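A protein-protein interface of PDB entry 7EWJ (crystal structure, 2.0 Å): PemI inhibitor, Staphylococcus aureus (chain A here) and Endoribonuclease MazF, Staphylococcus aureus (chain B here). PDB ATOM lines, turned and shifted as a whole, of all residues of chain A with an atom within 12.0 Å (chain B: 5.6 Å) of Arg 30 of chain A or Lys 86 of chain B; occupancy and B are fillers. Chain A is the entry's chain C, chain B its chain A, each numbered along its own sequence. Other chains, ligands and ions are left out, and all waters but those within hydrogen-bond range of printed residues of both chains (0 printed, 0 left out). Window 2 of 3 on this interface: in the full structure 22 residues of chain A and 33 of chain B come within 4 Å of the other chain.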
ATOM      1  N   GLU A  25      13.080   3.936  -7.976  1.00  0.00           N
ATOM      2  CA  GLU A  25      11.711   3.440  -8.126  1.00  0.00           C
ATOM      3  C   GLU A  25      11.620   2.098  -8.835  1.00  0.00           C
ATOM      4  O   GLU A  25      10.632   1.357  -8.648  1.00  0.00           O
ATOM      5  CB  GLU A  25      10.936   4.429  -9.020  1.00  0.00           C
ATOM      6  CG  GLU A  25      10.337   5.498  -8.274  1.00  0.00           C
ATOM      7  CD  GLU A  25       9.271   6.214  -9.074  1.00  0.00           C
ATOM      8  OE1 GLU A  25       8.288   6.574  -8.407  1.00  0.00           O
ATOM      9  OE2 GLU A  25       9.395   6.381 -10.327  1.00  0.00           O
ATOM     10  N   GLU A  26      12.510   1.847  -9.789  1.00  0.00           N
ATOM     11  CA  GLU A  26      12.316   0.686 -10.654  1.00  0.00           C
ATOM     12  C   GLU A  26      12.696  -0.601  -9.939  1.00  0.00           C
ATOM     13  O   GLU A  26      13.617  -0.623  -9.125  1.00  0.00           O
ATOM     14  CB  GLU A  26      13.144   0.809 -11.937  1.00  0.00           C
ATOM     15  CG  GLU A  26      12.707   1.909 -12.938  1.00  0.00           C
ATOM     16  CD  GLU A  26      11.230   1.739 -13.427  1.00  0.00           C
ATOM     17  OE1 GLU A  26      10.825   0.599 -13.784  1.00  0.00           O
ATOM     18  OE2 GLU A  26      10.493   2.748 -13.494  1.00  0.00           O
ATOM     19  N   ARG A  27      11.986  -1.686 -10.274  1.00  0.00           N
ATOM     20  CA  ARG A  27      12.244  -3.033  -9.745  1.00  0.00           C
ATOM     21  C   ARG A  27      12.697  -3.946 -10.880  1.00  0.00           C
ATOM     22  O   ARG A  27      12.137  -3.871 -11.972  1.00  0.00           O
ATOM     23  CB  ARG A  27      10.980  -3.597  -9.070  1.00  0.00           C
ATOM     24  CG  ARG A  27      10.618  -2.848  -7.750  1.00  0.00           C
ATOM     25  CD  ARG A  27       9.308  -3.379  -7.115  1.00  0.00           C
ATOM     26  NE  ARG A  27       8.149  -2.993  -7.943  1.00  0.00           N
ATOM     27  CZ  ARG A  27       6.908  -3.464  -7.754  1.00  0.00           C
ATOM     28  NH1 ARG A  27       6.644  -4.323  -6.757  1.00  0.00           N
ATOM     29  NH2 ARG A  27       5.938  -3.115  -8.584  1.00  0.00           N
ATOM     30  N   VAL A  28      13.760  -4.739 -10.661  1.00  0.00           N
ATOM     31  CA  VAL A  28      14.257  -5.697 -11.660  1.00  0.00           C
ATOM     32  C   VAL A  28      14.522  -7.032 -10.963  1.00  0.00           C
ATOM     33  O   VAL A  28      14.562  -7.106  -9.737  1.00  0.00           O
ATOM     34  CB  VAL A  28      15.533  -5.199 -12.379  1.00  0.00           C
ATOM     35  CG1 VAL A  28      15.230  -3.878 -13.091  1.00  0.00           C
ATOM     36  CG2 VAL A  28      16.669  -4.966 -11.365  1.00  0.00           C
ATOM     37  N   GLY A  29      14.755  -8.080 -11.762  1.00  0.00           N
ATOM     38  CA  GLY A  29      15.124  -9.383 -11.192  1.00  0.00           C
ATOM     39  C   GLY A  29      14.052  -9.903 -10.253  1.00  0.00           C
ATOM     40  O   GLY A  29      12.858  -9.893 -10.562  1.00  0.00           O
ATOM     41  N   ARG A  30      14.458 -10.302  -9.061  1.00  0.00           N
ATOM     42  CA  ARG A  30      13.527 -10.868  -8.098  1.00  0.00           C
ATOM     43  C   ARG A  30      12.882  -9.806  -7.212  1.00  0.00           C
ATOM     44  O   ARG A  30      12.171 -10.157  -6.276  1.00  0.00           O
ATOM     45  CB  ARG A  30      14.239 -11.915  -7.225  1.00  0.00           C
ATOM     46  CG  ARG A  30      14.940 -13.101  -8.051  1.00  0.00           C
ATOM     47  CD  ARG A  30      15.904 -13.877  -7.140  1.00  0.00           C
ATOM     48  NE  ARG A  30      17.134 -13.097  -6.904  1.00  0.00           N
ATOM     49  CZ  ARG A  30      17.880 -13.157  -5.797  1.00  0.00           C
ATOM     50  NH1 ARG A  30      17.559 -13.994  -4.807  1.00  0.00           N
ATOM     51  NH2 ARG A  30      18.969 -12.387  -5.676  1.00  0.00           N
ATOM     52  N   GLU A  31      13.122  -8.515  -7.467  1.00  0.00           N
ATOM     53  CA  GLU A  31      12.598  -7.474  -6.578  1.00  0.00           C
ATOM     54  C   GLU A  31      11.084  -7.378  -6.735  1.00  0.00           C
ATOM     55  O   GLU A  31      10.570  -7.428  -7.858  1.00  0.00           O
ATOM     56  CB  GLU A  31      13.227  -6.118  -6.918  1.00  0.00           C
ATOM     57  CG  GLU A  31      14.727  -6.047  -6.589  1.00  0.00           C
ATOM     58  CD  GLU A  31      15.420  -4.938  -7.327  1.00  0.00           C
ATOM     59  OE1 GLU A  31      14.714  -4.020  -7.854  1.00  0.00           O
ATOM     60  OE2 GLU A  31      16.673  -4.990  -7.398  1.00  0.00           O
ATOM     61  N   ILE A  32      10.369  -7.234  -5.614  1.00  0.00           N
ATOM     62  CA  ILE A  32       8.887  -7.188  -5.652  1.00  0.00           C
ATOM     63  C   ILE A  32       8.302  -6.030  -4.822  1.00  0.00           C
ATOM     64  O   ILE A  32       8.989  -5.445  -3.984  1.00  0.00           O
ATOM     65  CB  ILE A  32       8.238  -8.527  -5.188  1.00  0.00           C
ATOM     66  CG1 ILE A  32       8.531  -8.779  -3.716  1.00  0.00           C
ATOM     67  CG2 ILE A  32       8.586  -9.722  -6.143  1.00  0.00           C
ATOM     68  CD1 ILE A  32       7.974 -10.094  -3.195  1.00  0.00           C
ATOM     69  N   THR B  43      20.949 -14.471   0.268  1.00  0.00           N
ATOM     70  CA  THR B  43      19.857 -13.974  -0.608  1.00  0.00           C
ATOM     71  C   THR B  43      20.301 -13.381  -1.936  1.00  0.00           C
ATOM     72  O   THR B  43      19.483 -13.334  -2.873  1.00  0.00           O
ATOM     73  CB  THR B  43      19.043 -12.908   0.111  1.00  0.00           C
ATOM     74  OG1 THR B  43      19.859 -11.724   0.230  1.00  0.00           O
ATOM     75  CG2 THR B  43      18.650 -13.395   1.520  1.00  0.00           C
ATOM     76  N   ASN B  44      21.571 -12.941  -2.039  1.00  0.00           N
ATOM     77  CA  ASN B  44      22.117 -12.116  -3.126  1.00  0.00           C
ATOM     78  C   ASN B  44      21.344 -10.797  -3.305  1.00  0.00           C
ATOM     79  O   ASN B  44      21.274 -10.254  -4.416  1.00  0.00           O
ATOM     80  CB  ASN B  44      22.193 -12.867  -4.460  1.00  0.00           C
ATOM     81  CG  ASN B  44      23.278 -13.960  -4.488  1.00  0.00           C
ATOM     82  OD1 ASN B  44      23.001 -15.096  -4.817  1.00  0.00           O
ATOM     83  ND2 ASN B  44      24.460 -13.631  -4.087  1.00  0.00           N
ATOM     84  N   PHE B  45      20.776 -10.269  -2.214  1.00  0.00           N
ATOM     85  CA  PHE B  45      20.240  -8.917  -2.143  1.00  0.00           C
ATOM     86  C   PHE B  45      21.132  -8.108  -1.225  1.00  0.00           C
ATOM     87  O   PHE B  45      21.594  -8.604  -0.198  1.00  0.00           O
ATOM     88  CB  PHE B  45      18.826  -8.887  -1.503  1.00  0.00           C
ATOM     89  CG  PHE B  45      17.699  -9.180  -2.456  1.00  0.00           C
ATOM     90  CD1 PHE B  45      17.372 -10.506  -2.802  1.00  0.00           C
ATOM     91  CD2 PHE B  45      16.893  -8.131  -2.945  1.00  0.00           C
ATOM     92  CE1 PHE B  45      16.283 -10.783  -3.665  1.00  0.00           C
ATOM     93  CE2 PHE B  45      15.815  -8.380  -3.790  1.00  0.00           C
ATOM     94  CZ  PHE B  45      15.495  -9.705  -4.177  1.00  0.00           C
ATOM     95  N   ASP B  84      18.425  -6.500  -5.847  1.00  0.00           N
ATOM     96  CA  ASP B  84      18.838  -7.833  -6.305  1.00  0.00           C
ATOM     97  C   ASP B  84      20.131  -7.708  -7.127  1.00  0.00           C
ATOM     98  O   ASP B  84      20.095  -7.314  -8.289  1.00  0.00           O
ATOM     99  CB  ASP B  84      17.693  -8.422  -7.128  1.00  0.00           C
ATOM    100  CG  ASP B  84      18.011  -9.782  -7.721  1.00  0.00           C
ATOM    101  OD1 ASP B  84      19.119 -10.320  -7.504  1.00  0.00           O
ATOM    102  OD2 ASP B  84      17.119 -10.320  -8.398  1.00  0.00           O
ATOM    103  N   LEU B  85      21.281  -8.080  -6.553  1.00  0.00           N
ATOM    104  CA  LEU B  85      22.550  -7.854  -7.270  1.00  0.00           C
ATOM    105  C   LEU B  85      22.814  -8.917  -8.329  1.00  0.00           C
ATOM    106  O   LEU B  85      23.739  -8.759  -9.136  1.00  0.00           O
ATOM    107  CB  LEU B  85      23.734  -7.803  -6.284  1.00  0.00           C
ATOM    108  CG  LEU B  85      23.770  -6.504  -5.467  1.00  0.00           C
ATOM    109  CD1 LEU B  85      25.100  -6.241  -4.850  1.00  0.00           C
ATOM    110  CD2 LEU B  85      23.325  -5.276  -6.338  1.00  0.00           C
ATOM    111  N   LYS B  86      21.995  -9.974  -8.379  1.00  0.00           N
ATOM    112  CA  LYS B  86      22.017 -10.841  -9.552  1.00  0.00           C
ATOM    113  C   LYS B  86      21.458 -10.134 -10.775  1.00  0.00           C
ATOM    114  O   LYS B  86      21.690 -10.588 -11.898  1.00  0.00           O
ATOM    115  CB  LYS B  86      21.170 -12.107  -9.355  1.00  0.00           C
ATOM    116  CG  LYS B  86      21.767 -13.295  -8.683  1.00  0.00           C
ATOM    117  CD  LYS B  86      20.632 -14.089  -7.979  1.00  0.00           C
ATOM    118  CE  LYS B  86      21.065 -15.545  -7.627  1.00  0.00           C
ATOM    119  NZ  LYS B  86      20.538 -16.102  -6.313  1.00  0.00           N
ATOM    120  N   ALA B  87      20.674  -9.066 -10.602  1.00  0.00           N
ATOM    121  CA  ALA B  87      20.028  -8.429 -11.743  1.00  0.00           C
ATOM    122  C   ALA B  87      20.536  -7.034 -12.031  1.00  0.00           C
ATOM    123  O   ALA B  87      20.031  -6.392 -12.951  1.00  0.00           O
ATOM    124  CB  ALA B  87      18.501  -8.371 -11.527  1.00  0.00           C
ATOM    125  N   ARG B  88      21.435  -6.489 -11.221  1.00  0.00           N
ATOM    126  CA  ARG B  88      21.871  -5.114 -11.425  1.00  0.00           C
ATOM    127  C   ARG B  88      23.389  -5.084 -11.507  1.00  0.00           C
ATOM    128  O   ARG B  88      24.036  -5.803 -10.756  1.00  0.00           O
ATOM    129  CB  ARG B  88      21.413  -4.189 -10.272  1.00  0.00           C
ATOM    130  CG  ARG B  88      19.895  -4.022 -10.168  1.00  0.00           C
ATOM    131  CD  ARG B  88      19.581  -3.257  -8.943  1.00  0.00           C
ATOM    132  NE  ARG B  88      18.141  -3.091  -8.743  1.00  0.00           N
ATOM    133  CZ  ARG B  88      17.453  -2.073  -9.226  1.00  0.00           C
ATOM    134  NH1 ARG B  88      18.082  -1.156  -9.948  1.00  0.00           N
ATOM    135  NH2 ARG B  88      16.165  -1.983  -8.959  1.00  0.00           N
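Of the 8 printed residues of chain A, 5 touch a printed residue of chain B.
Printed residues of chain A that touch a printed residue of chain B: Glu 26, Val 28, Gly 29, Arg 30 and Glu 31.
Along chain A the printed residues that touch a printed residue of chain B span positions 26 to 31.
Of the 8 printed residues of chain B, 7 touch a printed residue of chain A.
Along chain B the printed residues that touch a printed residue of chain A span positions 43 to 88.
Among the printed residues, 13 pairs touch across the chains.
Among the printed residues, Asp or Glu carboxylates within 4 Å of a Lys or Arg side-chain nitrogen of the other chain: Arg 30 of chain A with Asp 84 of chain B and Glu 31 of chain A with Arg 88 of chain B.
Glu 25 of chain A touches none of the printed residues of chain B.
Of the printed residues of chain B, Glu 26 of chain A touches Arg 88.
Of the printed residues of chain B, Val 28 of chain A touches Ala 87 and Arg 88.
Of the printed residues of chain B, Gly 29 of chain A touches Asp 84 and Ala 87.
Printed residues of chain B within 4 Å of Arg 30 of chain A: Thr 43, Asn 44, Phe 45, Asp 84 and Lys 86.
Thr 43 of chain B touches just one residue of chain A: Arg 30 (2.8 Å).
Printed residues of chain A within 4 Å of Asn 44 of chain B: Arg 30 (3.4 Å).
Phe 45 of chain B touches just these residues of chain A: Arg 30 and Glu 31.
Asp 84 of chain B touches three residues of chain A.
No residue of chain A comes within 4 Å of Leu 85 of chain B.
Lys 86 of chain B touches just one residue of chain A: Arg 30.
The nearest residue of chain B that does not touch Arg 30 of chain A is Leu 85 of chain B (5.0 Å).
The nearest residue of chain A that does not touch Lys 86 of chain B is Gly 29 of chain A (6.4 Å).
The nearest printed residue of chain B that does not touch Gly 29 of chain A is Phe 45 of chain B (6.2 Å).
NH1 of Arg 30 of chain A is in hydrogen-bond range of O of Thr 43 of chain B.
The backbone carbonyl oxygen (O) of Asn 44 of chain B sits at hydrogen-bond distance from the guanidinium group (NH2) of Arg 30 of chain A.
The side-chain carboxylate (OD1) of Asp 84 of chain B lies within salt-bridge range of the guanidinium group (NH2) of Arg 30 of chain A (2.8 Å).
N of Asp 84 of chain B sits at hydrogen-bond distance from OE2 of Glu 31 of chain A (2.8 Å).
O of Glu 26 of chain A lies within hydrogen-bond range of NH2 of Arg 88 of chain B.
OE1 of Glu 31 of chain A is in salt-bridge range of NH2 of Arg 88 of chain B (2.7 Å).
Among the printed residues, merely in contact across the chains: Arg 30 of chain A with Lys 86 of chain B (3.3 Å), Gly 29 of chain A with Ala 87 of chain B (3.5 Å), Val 28 of chain A with Arg 88 of chain B (3.5 Å), Gly 29 of chain A with Asp 84 of chain B (3.6 Å), Arg 30 of chain A with Phe 45 of chain B (3.6 Å), Glu 31 of chain A with Phe 45 of chain B (3.8 Å) and Val 28 of chain A with Ala 87 of chain B (3.9 Å).
The side-chain hydroxyl (OG1) of Thr 43 of chain B is in hydrogen-bond range of the backbone NH (N) of Phe 45 of chain B, at 3.0 Å.
The backbone NH of Leu 85 of chain B sits at hydrogen-bond distance from the backbone carbonyl oxygen of Asn 44 of chain B, 3.0 Å away.
The side-chain amide oxygen (OD1) of Asn 44 of chain B lies within hydrogen-bond range of the side-chain amino group (NZ) of Lys 86 of chain B.
OD1 of Asp 84 of chain B sits at hydrogen-bond distance from N of Lys 86 of chain B (3.0 Å).
The backbone NH (N) of Val 28 of chain A is in hydrogen-bond range of the side-chain carboxylate (OE1) of Glu 31 of chain A, at 3.1 Å.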
